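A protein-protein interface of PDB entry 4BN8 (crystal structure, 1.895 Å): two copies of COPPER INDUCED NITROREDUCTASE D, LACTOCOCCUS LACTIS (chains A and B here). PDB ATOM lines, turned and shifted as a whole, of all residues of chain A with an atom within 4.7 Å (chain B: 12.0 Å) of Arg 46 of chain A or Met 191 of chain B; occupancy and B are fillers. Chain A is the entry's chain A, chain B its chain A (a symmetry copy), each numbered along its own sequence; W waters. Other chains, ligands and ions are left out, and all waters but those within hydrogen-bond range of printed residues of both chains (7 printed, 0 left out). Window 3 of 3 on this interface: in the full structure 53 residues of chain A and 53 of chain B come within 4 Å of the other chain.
NH1 of Arg 34 of chain A lies within salt-bridge range of OD1 of Asp 193 of chain B, 3.7 Å away. OE1 of Gln 43 of chain A lies within hydrogen-bond range of N of Met 191 of chain B, at 2.8 Å. The side-chain amide oxygen (OE1) of Gln 43 of chain A sits at hydrogen-bond distance from the guanidinium group (NH2) of Arg 196 of chain B, 3.4 Å away. The side-chain sulfur (SD) of Met 191 of chain B sits at hydrogen-bond distance from the guanidinium group (NH1) of Arg 46 of chain A, 3.5 Å away. N of Leu 47 of chain A is in hydrogen-bond range of O of Arg 196 of chain B, at 2.8 Å. O of Leu 47 of chain A lies within hydrogen-bond range of N of Ile 198 of chain B (2.9 Å).
The backbone carbonyl oxygen of Gln 43 of chain A lies within hydrogen-bond range of the guanidinium group of Arg 46 of chain A (2.8 Å). O of Arg 46 of chain A sits at hydrogen-bond distance from N of Phe 101 of chain A, at 2.8 Å. NE of Arg 46 of chain A lies within salt-bridge range of OD2 of Asp 103 of chain A, 3.1 Å away. O of Leu 48 of chain A lies within hydrogen-bond range of N of Leu 99 of chain A (2.8 Å).
Among the printed residues, pairs that only touch across the chains: Arg 34 of chain A with Phe 190 of chain B (3.4 Å), Arg 34 of chain A with Arg 196 of chain B (3.7 Å), Gln 43 of chain A with Thr 189 of chain B (3.8 Å), Gln 43 of chain A with Phe 190 of chain B (3.5 Å), Gly 45 of chain A with Arg 196 of chain B (3.7 Å), Arg 46 of chain A with Asp 195 of chain B (3.6 Å), Arg 46 of chain A with Arg 196 of chain B (3.5 Å), Leu 47 of chain A with Phe 197 of chain B (3.7 Å), Leu 48 of chain A with Ile 198 of chain B (3.4 Å) and Trp 170 of chain A with Ile 198 of chain B (3.7 Å).
Of chain B, only Thr 189, Phe 190, Met 191 and Arg 196 come within 4 Å of Gln 43 of chain A. No residue of chain B comes within 4 Å of Thr 44 of chain A. Arg 46 of chain A touches just these residues of chain B: Met 191 (3.5 Å), Asp 195 (3.6 Å) and Arg 196 (3.5 Å). Leu 47 of chain A touches three residues of chain B. No residue of chain B comes within 4 Å of Phe 100 of chain A. No residue of chain B comes within 4 Å of Phe 101 of chain A. No residue of chain B comes within 4 Å of Asp 103 of chain A. Of chain B, only Ile 198 comes within 4 Å of Trp 170 of chain A. Printed residues of chain A within 4 Å of Thr 189 of chain B: Gln 43 (3.8 Å). Printed residues of chain A within 4 Å of Phe 190 of chain B: Arg 34 (3.4 Å) and Gln 43 (3.5 Å). Of chain A, only Gln 43 (2.8 Å) and Arg 46 (3.5 Å) come within 4 Å of Met 191 of chain B. Asp 192 of chain B touches none of the printed residues of chain A. Of the printed residues of chain A, Asp 193 of chain B touches Arg 34 (3.7 Å). Of the printed residues of chain A, Asp 195 of chain B touches Arg 46 (3.6 Å). Of the printed residues of chain A, Phe 197 of chain B touches Leu 47.
Among the printed residues, 16 pairs touch across the chains.
No position is printed for both chains. Of the 16 pairs that touch across the chains among the printed residues, none has its exchanged pair printed and touching as well.
Water W6 lies within hydrogen-bond range of NH1 of Arg 196 of chain B and O of Gly 45 of chain A. Water W7 lies within hydrogen-bond range of OD1 of Asp 193 of chain B (2.8 Å) and NH1 of Arg 34 of chain A (3.1 Å). Water W2 lies within hydrogen-bond range of OG1 of Thr 189 of chain B (2.8 Å) and NE2 of Gln 43 of chain A (3.0 Å). Water W5 lies within hydrogen-bond range of the backbone carbonyl oxygen of Gln 43 of chain A (2.9 Å), the guanidinium group of Arg 46 of chain A (2.9 Å) and the side-chain sulfur of Met 191 of chain B (3.4 Å). Water W3 lies within hydrogen-bond range of the side-chain amino group (NZ) of Lys 188 of chain B (2.9 Å) and the backbone carbonyl oxygen (O) of Arg 34 of chain A (3.0 Å). Water W1 bridges O of Thr 189 of chain B (2.9 Å) and OE1 of Gln 43 of chain A (3.4 Å).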
ATOM      1  N   ARG A  34      12.055  17.353 -14.769  1.00  0.00           N
ATOM      2  CA  ARG A  34      13.464  17.137 -15.049  1.00  0.00           C
ATOM      3  C   ARG A  34      13.987  15.859 -14.404  1.00  0.00           C
ATOM      4  O   ARG A  34      14.699  15.072 -15.036  1.00  0.00           O
ATOM      5  CB  ARG A  34      14.274  18.329 -14.545  1.00  0.00           C
ATOM      6  CG  ARG A  34      15.761  18.202 -14.743  1.00  0.00           C
ATOM      7  CD  ARG A  34      16.499  19.407 -14.171  1.00  0.00           C
ATOM      8  NE  ARG A  34      17.879  19.476 -14.650  1.00  0.00           N
ATOM      9  CZ  ARG A  34      18.254  20.054 -15.791  1.00  0.00           C
ATOM     10  NH1 ARG A  34      17.354  20.618 -16.588  1.00  0.00           N
ATOM     11  NH2 ARG A  34      19.535  20.060 -16.141  1.00  0.00           N
ATOM     12  N   GLN A  43      12.915  11.377 -22.412  1.00  0.00           N
ATOM     13  CA  GLN A  43      12.390  12.686 -22.017  1.00  0.00           C
ATOM     14  C   GLN A  43      11.331  13.180 -22.998  1.00  0.00           C
ATOM     15  O   GLN A  43      11.460  14.257 -23.584  1.00  0.00           O
ATOM     16  CB  GLN A  43      13.539  13.692 -21.937  1.00  0.00           C
ATOM     17  CG  GLN A  43      14.545  13.383 -20.843  1.00  0.00           C
ATOM     18  CD  GLN A  43      15.813  14.194 -20.983  1.00  0.00           C
ATOM     19  OE1 GLN A  43      15.882  15.344 -20.540  1.00  0.00           O
ATOM     20  NE2 GLN A  43      16.824  13.604 -21.614  1.00  0.00           N
ATOM     21  N   THR A  44      10.287  12.376 -23.171  1.00  0.00           N
ATOM     22  CA  THR A  44       9.291  12.611 -24.203  1.00  0.00           C
ATOM     23  C   THR A  44       8.214  13.601 -23.761  1.00  0.00           C
ATOM     24  O   THR A  44       7.407  14.042 -24.579  1.00  0.00           O
ATOM     25  CB  THR A  44       8.605  11.305 -24.610  1.00  0.00           C
ATOM     26  OG1 THR A  44       8.205  10.584 -23.433  1.00  0.00           O
ATOM     27  CG2 THR A  44       9.546  10.456 -25.447  1.00  0.00           C
ATOM     28  N   GLY A  45       8.208  13.948 -22.475  1.00  0.00           N
ATOM     29  CA  GLY A  45       7.195  14.828 -21.927  1.00  0.00           C
ATOM     30  C   GLY A  45       7.393  16.263 -22.370  1.00  0.00           C
ATOM     31  O   GLY A  45       8.526  16.746 -22.459  1.00  0.00           O
ATOM     32  N   ARG A  46       6.284  16.938 -22.657  1.00  0.00           N
ATOM     33  CA  ARG A  46       6.302  18.350 -23.025  1.00  0.00           C
ATOM     34  C   ARG A  46       5.207  19.068 -22.237  1.00  0.00           C
ATOM     35  O   ARG A  46       4.133  18.512 -22.026  1.00  0.00           O
ATOM     36  CB  ARG A  46       6.059  18.519 -24.521  1.00  0.00           C
ATOM     37  CG  ARG A  46       6.989  17.707 -25.422  1.00  0.00           C
ATOM     38  CD  ARG A  46       8.323  18.386 -25.623  1.00  0.00           C
ATOM     39  NE  ARG A  46       9.202  17.601 -26.484  1.00  0.00           N
ATOM     40  CZ  ARG A  46      10.050  16.671 -26.045  1.00  0.00           C
ATOM     41  NH1 ARG A  46      10.144  16.397 -24.750  1.00  0.00           N
ATOM     42  NH2 ARG A  46      10.806  16.010 -26.907  1.00  0.00           N
ATOM     43  N   LEU A  47       5.476  20.294 -21.797  1.00  0.00           N
ATOM     44  CA  LEU A  47       4.509  21.024 -20.985  1.00  0.00           C
ATOM     45  C   LEU A  47       4.182  22.392 -21.554  1.00  0.00           C
ATOM     46  O   LEU A  47       5.062  23.109 -22.032  1.00  0.00           O
ATOM     47  CB  LEU A  47       5.018  21.212 -19.558  1.00  0.00           C
ATOM     48  CG  LEU A  47       4.767  20.083 -18.557  1.00  0.00           C
ATOM     49  CD1 LEU A  47       5.556  18.839 -18.918  1.00  0.00           C
ATOM     50  CD2 LEU A  47       5.124  20.563 -17.164  1.00  0.00           C
ATOM     51  N   LEU A  48       2.902  22.733 -21.495  1.00  0.00           N
ATOM     52  CA  LEU A  48       2.450  24.097 -21.698  1.00  0.00           C
ATOM     53  C   LEU A  48       1.859  24.576 -20.370  1.00  0.00           C
ATOM     54  O   LEU A  48       0.890  24.009 -19.869  1.00  0.00           O
ATOM     55  CB  LEU A  48       1.406  24.156 -22.815  1.00  0.00           C
ATOM     56  CG  LEU A  48       0.735  25.515 -23.055  1.00  0.00           C
ATOM     57  CD1 LEU A  48       1.755  26.570 -23.452  1.00  0.00           C
ATOM     58  CD2 LEU A  48      -0.351  25.399 -24.117  1.00  0.00           C
ATOM     59  N   LEU A  99      -0.657  21.745 -19.120  1.00  0.00           N
ATOM     60  CA  LEU A  99      -1.043  20.768 -20.126  1.00  0.00           C
ATOM     61  C   LEU A  99       0.146  19.876 -20.454  1.00  0.00           C
ATOM     62  O   LEU A  99       1.203  20.353 -20.869  1.00  0.00           O
ATOM     63  CB  LEU A  99      -1.567  21.456 -21.387  1.00  0.00           C
ATOM     64  CG  LEU A  99      -2.834  22.300 -21.192  1.00  0.00           C
ATOM     65  CD1 LEU A  99      -2.492  23.721 -20.772  1.00  0.00           C
ATOM     66  CD2 LEU A  99      -3.679  22.312 -22.452  1.00  0.00           C
ATOM     67  N   PHE A 100      -0.043  18.579 -20.253  1.00  0.00           N
ATOM     68  CA  PHE A 100       1.001  17.591 -20.479  1.00  0.00           C
ATOM     69  C   PHE A 100       0.843  16.934 -21.839  1.00  0.00           C
ATOM     70  O   PHE A 100      -0.226  16.413 -22.153  1.00  0.00           O
ATOM     71  CB  PHE A 100       0.935  16.520 -19.389  1.00  0.00           C
ATOM     72  CG  PHE A 100       1.374  17.003 -18.045  1.00  0.00           C
ATOM     73  CD1 PHE A 100       2.705  16.941 -17.676  1.00  0.00           C
ATOM     74  CD2 PHE A 100       0.457  17.526 -17.146  1.00  0.00           C
ATOM     75  CE1 PHE A 100       3.113  17.391 -16.438  1.00  0.00           C
ATOM     76  CE2 PHE A 100       0.863  17.979 -15.914  1.00  0.00           C
ATOM     77  CZ  PHE A 100       2.191  17.908 -15.556  1.00  0.00           C
ATOM     78  N   PHE A 101       1.907  16.961 -22.641  1.00  0.00           N
ATOM     79  CA  PHE A 101       1.920  16.285 -23.937  1.00  0.00           C
ATOM     80  C   PHE A 101       3.045  15.249 -23.972  1.00  0.00           C
ATOM     81  O   PHE A 101       3.932  15.262 -23.122  1.00  0.00           O
ATOM     82  CB  PHE A 101       2.168  17.268 -25.087  1.00  0.00           C
ATOM     83  CG  PHE A 101       1.268  18.467 -25.093  1.00  0.00           C
ATOM     84  CD1 PHE A 101       1.409  19.466 -24.144  1.00  0.00           C
ATOM     85  CD2 PHE A 101       0.308  18.617 -26.079  1.00  0.00           C
ATOM     86  CE1 PHE A 101       0.591  20.577 -24.161  1.00  0.00           C
ATOM     87  CE2 PHE A 101      -0.515  19.733 -26.101  1.00  0.00           C
ATOM     88  CZ  PHE A 101      -0.366  20.714 -25.141  1.00  0.00           C
ATOM     89  N   ASP A 103       5.838  13.826 -26.881  1.00  0.00           N
ATOM     90  CA  ASP A 103       6.373  14.130 -28.209  1.00  0.00           C
ATOM     91  C   ASP A 103       6.439  12.870 -29.061  1.00  0.00           C
ATOM     92  O   ASP A 103       7.291  12.009 -28.849  1.00  0.00           O
ATOM     93  CB  ASP A 103       7.761  14.750 -28.089  1.00  0.00           C
ATOM     94  CG  ASP A 103       8.219  15.404 -29.374  1.00  0.00           C
ATOM     95  OD1 ASP A 103       7.912  14.868 -30.459  1.00  0.00           O
ATOM     96  OD2 ASP A 103       8.879  16.459 -29.296  1.00  0.00           O
ATOM     97  N   VAL A 106       9.728  11.947 -31.109  1.00  0.00           N
ATOM     98  CA  VAL A 106      10.766  11.226 -30.393  1.00  0.00           C
ATOM     99  C   VAL A 106      10.394   9.750 -30.314  1.00  0.00           C
ATOM    100  O   VAL A 106      11.218   8.879 -30.571  1.00  0.00           O
ATOM    101  CB  VAL A 106      10.961  11.793 -28.979  1.00  0.00           C
ATOM    102  CG1 VAL A 106      11.949  10.939 -28.199  1.00  0.00           C
ATOM    103  CG2 VAL A 106      11.427  13.243 -29.054  1.00  0.00           C
ATOM    104  N   TRP A 170       3.345  17.169 -30.612  1.00  0.00           N
ATOM    105  CA  TRP A 170       2.957  17.140 -29.204  1.00  0.00           C
ATOM    106  C   TRP A 170       1.553  16.555 -29.023  1.00  0.00           C
ATOM    107  O   TRP A 170       0.559  17.181 -29.395  1.00  0.00           O
ATOM    108  CB  TRP A 170       2.989  18.542 -28.604  1.00  0.00           C
ATOM    109  CG  TRP A 170       4.356  19.114 -28.392  1.00  0.00           C
ATOM    110  CD1 TRP A 170       5.509  18.769 -29.037  1.00  0.00           C
ATOM    111  CD2 TRP A 170       4.709  20.143 -27.464  1.00  0.00           C
ATOM    112  NE1 TRP A 170       6.556  19.521 -28.565  1.00  0.00           N
ATOM    113  CE2 TRP A 170       6.090  20.372 -27.598  1.00  0.00           C
ATOM    114  CE3 TRP A 170       3.987  20.893 -26.530  1.00  0.00           C
ATOM    115  CZ2 TRP A 170       6.763  21.324 -26.837  1.00  0.00           C
ATOM    116  CZ3 TRP A 170       4.660  21.829 -25.772  1.00  0.00           C
ATOM    117  CH2 TRP A 170       6.030  22.041 -25.932  1.00  0.00           C
ATOM    118  N   GLN B 127      -0.727   4.526 -17.487  1.00  0.00           N
ATOM    119  CA  GLN B 127      -0.208   5.666 -16.739  1.00  0.00           C
ATOM    120  C   GLN B 127      -0.068   5.305 -15.260  1.00  0.00           C
ATOM    121  O   GLN B 127       0.959   5.592 -14.637  1.00  0.00           O
ATOM    122  CB  GLN B 127      -1.109   6.896 -16.946  1.00  0.00           C
ATOM    123  CG  GLN B 127      -1.013   7.453 -18.377  1.00  0.00           C
ATOM    124  CD  GLN B 127      -1.995   8.562 -18.680  1.00  0.00           C
ATOM    125  OE1 GLN B 127      -2.786   8.967 -17.828  1.00  0.00           O
ATOM    126  NE2 GLN B 127      -1.956   9.057 -19.913  1.00  0.00           N
ATOM    127  N   GLU B 187      26.463   8.701 -15.451  1.00  0.00           N
ATOM    128  CA  GLU B 187      26.133  10.059 -15.870  1.00  0.00           C
ATOM    129  C   GLU B 187      24.795  10.103 -16.602  1.00  0.00           C
ATOM    130  O   GLU B 187      24.394   9.133 -17.242  1.00  0.00           O
ATOM    131  CB  GLU B 187      27.238  10.598 -16.782  1.00  0.00           C
ATOM    132  CG  GLU B 187      28.591  10.720 -16.103  1.00  0.00           C
ATOM    133  CD  GLU B 187      29.740  10.852 -17.091  1.00  0.00           C
ATOM    134  OE1 GLU B 187      29.486  11.008 -18.306  1.00  0.00           O
ATOM    135  OE2 GLU B 187      30.905  10.796 -16.648  1.00  0.00           O
ATOM    136  N   LYS B 188      24.102  11.233 -16.500  1.00  0.00           N
ATOM    137  CA  LYS B 188      22.834  11.416 -17.197  1.00  0.00           C
ATOM    138  C   LYS B 188      22.744  12.843 -17.714  1.00  0.00           C
ATOM    139  O   LYS B 188      23.156  13.780 -17.033  1.00  0.00           O
ATOM    140  CB  LYS B 188      21.647  11.111 -16.274  1.00  0.00           C
ATOM    141  CG  LYS B 188      20.298  11.294 -16.942  1.00  0.00           C
ATOM    142  CD  LYS B 188      19.134  10.857 -16.052  1.00  0.00           C
ATOM    143  CE  LYS B 188      19.135  11.559 -14.706  1.00  0.00           C
ATOM    144  NZ  LYS B 188      17.825  11.346 -14.018  1.00  0.00           N
ATOM    145  N   THR B 189      22.236  13.004 -18.932  1.00  0.00           N
ATOM    146  CA  THR B 189      22.058  14.327 -19.511  1.00  0.00           C
ATOM    147  C   THR B 189      20.590  14.753 -19.447  1.00  0.00           C
ATOM    148  O   THR B 189      19.699  13.944 -19.179  1.00  0.00           O
ATOM    149  CB  THR B 189      22.529  14.382 -20.980  1.00  0.00           C
ATOM    150  OG1 THR B 189      21.810  13.413 -21.746  1.00  0.00           O
ATOM    151  CG2 THR B 189      24.036  14.110 -21.088  1.00  0.00           C
ATOM    152  N   PHE B 190      20.347  16.032 -19.695  1.00  0.00           N
ATOM    153  CA  PHE B 190      18.993  16.569 -19.687  1.00  0.00           C
ATOM    154  C   PHE B 190      18.787  17.421 -20.930  1.00  0.00           C
ATOM    155  O   PHE B 190      19.710  18.090 -21.394  1.00  0.00           O
ATOM    156  CB  PHE B 190      18.755  17.437 -18.449  1.00  0.00           C
ATOM    157  CG  PHE B 190      18.987  16.729 -17.145  1.00  0.00           C
ATOM    158  CD1 PHE B 190      20.255  16.668 -16.593  1.00  0.00           C
ATOM    159  CD2 PHE B 190      17.930  16.150 -16.456  1.00  0.00           C
ATOM    160  CE1 PHE B 190      20.480  16.026 -15.395  1.00  0.00           C
ATOM    161  CE2 PHE B 190      18.139  15.511 -15.243  1.00  0.00           C
ATOM    162  CZ  PHE B 190      19.419  15.445 -14.712  1.00  0.00           C
ATOM    163  N   MET B 191      17.568  17.395 -21.456  1.00  0.00           N
ATOM    164  CA  MET B 191      17.163  18.284 -22.536  1.00  0.00           C
ATOM    165  C   MET B 191      17.326  19.745 -22.159  1.00  0.00           C
ATOM    166  O   MET B 191      17.393  20.093 -20.980  1.00  0.00           O
ATOM    167  CB  MET B 191      15.680  18.103 -22.829  1.00  0.00           C
ATOM    168  CG  MET B 191      15.295  16.855 -23.559  1.00  0.00           C
ATOM    169  SD  MET B 191      13.516  16.900 -23.803  1.00  0.00           S
ATOM    170  CE  MET B 191      13.368  18.245 -24.984  1.00  0.00           C
ATOM    171  N   ASP B 192      17.338  20.600 -23.177  1.00  0.00           N
ATOM    172  CA  ASP B 192      17.210  22.039 -22.992  1.00  0.00           C
ATOM    173  C   ASP B 192      15.792  22.354 -22.510  1.00  0.00           C
ATOM    174  O   ASP B 192      14.816  21.898 -23.108  1.00  0.00           O
ATOM    175  CB  ASP B 192      17.470  22.734 -24.326  1.00  0.00           C
ATOM    176  CG  ASP B 192      17.532  24.247 -24.207  1.00  0.00           C
ATOM    177  OD1 ASP B 192      17.032  24.804 -23.208  1.00  0.00           O
ATOM    178  OD2 ASP B 192      18.073  24.880 -25.131  1.00  0.00           O
ATOM    179  N   ASP B 193      15.672  23.119 -21.425  1.00  0.00           N
ATOM    180  CA  ASP B 193      14.359  23.523 -20.927  1.00  0.00           C
ATOM    181  C   ASP B 193      13.513  24.114 -22.049  1.00  0.00           C
ATOM    182  O   ASP B 193      12.305  23.888 -22.112  1.00  0.00           O
ATOM    183  CB  ASP B 193      14.485  24.572 -19.821  1.00  0.00           C
ATOM    184  CG  ASP B 193      14.904  23.982 -18.487  1.00  0.00           C
ATOM    185  OD1 ASP B 193      14.913  22.738 -18.337  1.00  0.00           O
ATOM    186  OD2 ASP B 193      15.204  24.785 -17.577  1.00  0.00           O
ATOM    187  N   ALA B 194      14.150  24.890 -22.922  1.00  0.00           N
ATOM    188  CA  ALA B 194      13.422  25.630 -23.948  1.00  0.00           C
ATOM    189  C   ALA B 194      12.720  24.694 -24.925  1.00  0.00           C
ATOM    190  O   ALA B 194      11.772  25.092 -25.605  1.00  0.00           O
ATOM    191  CB  ALA B 194      14.362  26.580 -24.697  1.00  0.00           C
ATOM    192  N   ASP B 195      13.178  23.450 -24.993  1.00  0.00           N
ATOM    193  CA  ASP B 195      12.612  22.502 -25.941  1.00  0.00           C
ATOM    194  C   ASP B 195      11.450  21.693 -25.365  1.00  0.00           C
ATOM    195  O   ASP B 195      10.794  20.965 -26.106  1.00  0.00           O
ATOM    196  CB  ASP B 195      13.691  21.549 -26.452  1.00  0.00           C
ATOM    197  CG  ASP B 195      14.719  22.246 -27.329  1.00  0.00           C
ATOM    198  OD1 ASP B 195      14.348  23.183 -28.062  1.00  0.00           O
ATOM    199  OD2 ASP B 195      15.901  21.857 -27.276  1.00  0.00           O
ATOM    200  N   ARG B 196      11.189  21.795 -24.064  1.00  0.00           N
ATOM    201  CA  ARG B 196      10.086  21.014 -23.492  1.00  0.00           C
ATOM    202  C   ARG B 196       9.145  21.756 -22.542  1.00  0.00           C
ATOM    203  O   ARG B 196       8.114  21.203 -22.161  1.00  0.00           O
ATOM    204  CB  ARG B 196      10.598  19.731 -22.823  1.00  0.00           C
ATOM    205  CG  ARG B 196      11.534  19.924 -21.651  1.00  0.00           C
ATOM    206  CD  ARG B 196      11.790  18.574 -20.970  1.00  0.00           C
ATOM    207  NE  ARG B 196      12.934  18.605 -20.069  1.00  0.00           N
ATOM    208  CZ  ARG B 196      13.365  17.562 -19.366  1.00  0.00           C
ATOM    209  NH1 ARG B 196      12.737  16.399 -19.439  1.00  0.00           N
ATOM    210  NH2 ARG B 196      14.420  17.684 -18.578  1.00  0.00           N
ATOM    211  N   PHE B 197       9.480  22.991 -22.168  1.00  0.00           N
ATOM    212  CA  PHE B 197       8.585  23.803 -21.347  1.00  0.00           C
ATOM    213  C   PHE B 197       8.230  25.111 -22.050  1.00  0.00           C
ATOM    214  O   PHE B 197       9.114  25.871 -22.439  1.00  0.00           O
ATOM    215  CB  PHE B 197       9.218  24.130 -19.990  1.00  0.00           C
ATOM    216  CG  PHE B 197       9.732  22.931 -19.241  1.00  0.00           C
ATOM    217  CD1 PHE B 197       8.856  22.020 -18.673  1.00  0.00           C
ATOM    218  CD2 PHE B 197      11.095  22.735 -19.078  1.00  0.00           C
ATOM    219  CE1 PHE B 197       9.331  20.928 -17.970  1.00  0.00           C
ATOM    220  CE2 PHE B 197      11.579  21.645 -18.385  1.00  0.00           C
ATOM    221  CZ  PHE B 197      10.699  20.739 -17.828  1.00  0.00           C
ATOM    222  N   ILE B 198       6.930  25.355 -22.208  1.00  0.00           N
ATOM    223  CA  ILE B 198       6.426  26.643 -22.671  1.00  0.00           C
ATOM    224  C   ILE B 198       5.575  27.260 -21.571  1.00  0.00           C
ATOM    225  O   ILE B 198       4.642  26.632 -21.072  1.00  0.00           O
ATOM    226  CB  ILE B 198       5.556  26.507 -23.931  1.00  0.00           C
ATOM    227  CG1 ILE B 198       6.383  25.966 -25.097  1.00  0.00           C
ATOM    228  CG2 ILE B 198       4.949  27.867 -24.314  1.00  0.00           C
ATOM    229  CD1 ILE B 198       5.568  25.645 -26.333  1.00  0.00           C
ATOM    230  N   VAL B 199       5.908  28.487 -21.192  1.00  0.00           N
ATOM    231  CA  VAL B 199       5.151  29.207 -20.181  1.00  0.00           C
ATOM    232  C   VAL B 199       4.481  30.408 -20.831  1.00  0.00           C
ATOM    233  O   VAL B 199       5.139  31.206 -21.496  1.00  0.00           O
ATOM    234  CB  VAL B 199       6.059  29.684 -19.035  1.00  0.00           C
ATOM    235  CG1 VAL B 199       5.251  30.432 -17.991  1.00  0.00           C
ATOM    236  CG2 VAL B 199       6.794  28.509 -18.416  1.00  0.00           C
ATOM    237  N   ALA B 200       3.172  30.526 -20.644  1.00  0.00           N
ATOM    238  CA  ALA B 200       2.411  31.631 -21.207  1.00  0.00           C
ATOM    239  C   ALA B 200       1.541  32.287 -20.137  1.00  0.00           C
ATOM    240  O   ALA B 200       0.911  31.606 -19.323  1.00  0.00           O
ATOM    241  CB  ALA B 200       1.551  31.144 -22.364  1.00  0.00           C
HETATM  242  O   HOH W   1      17.063  13.343 -18.072  1.00  0.00           O
HETATM  243  O   HOH W   2      19.432  14.389 -22.851  1.00  0.00           O
HETATM  244  O   HOH W   3      15.668  12.346 -15.701  1.00  0.00           O
HETATM  245  O   HOH W   4      14.818  14.975 -17.710  1.00  0.00           O
HETATM  246  O   HOH W   5      12.991  14.331 -25.994  1.00  0.00           O
HETATM  247  O   HOH W   6      10.273  15.756 -20.495  1.00  0.00           O
HETATM  248  O   HOH W   7      14.542  21.697 -15.798  1.00  0.00           O
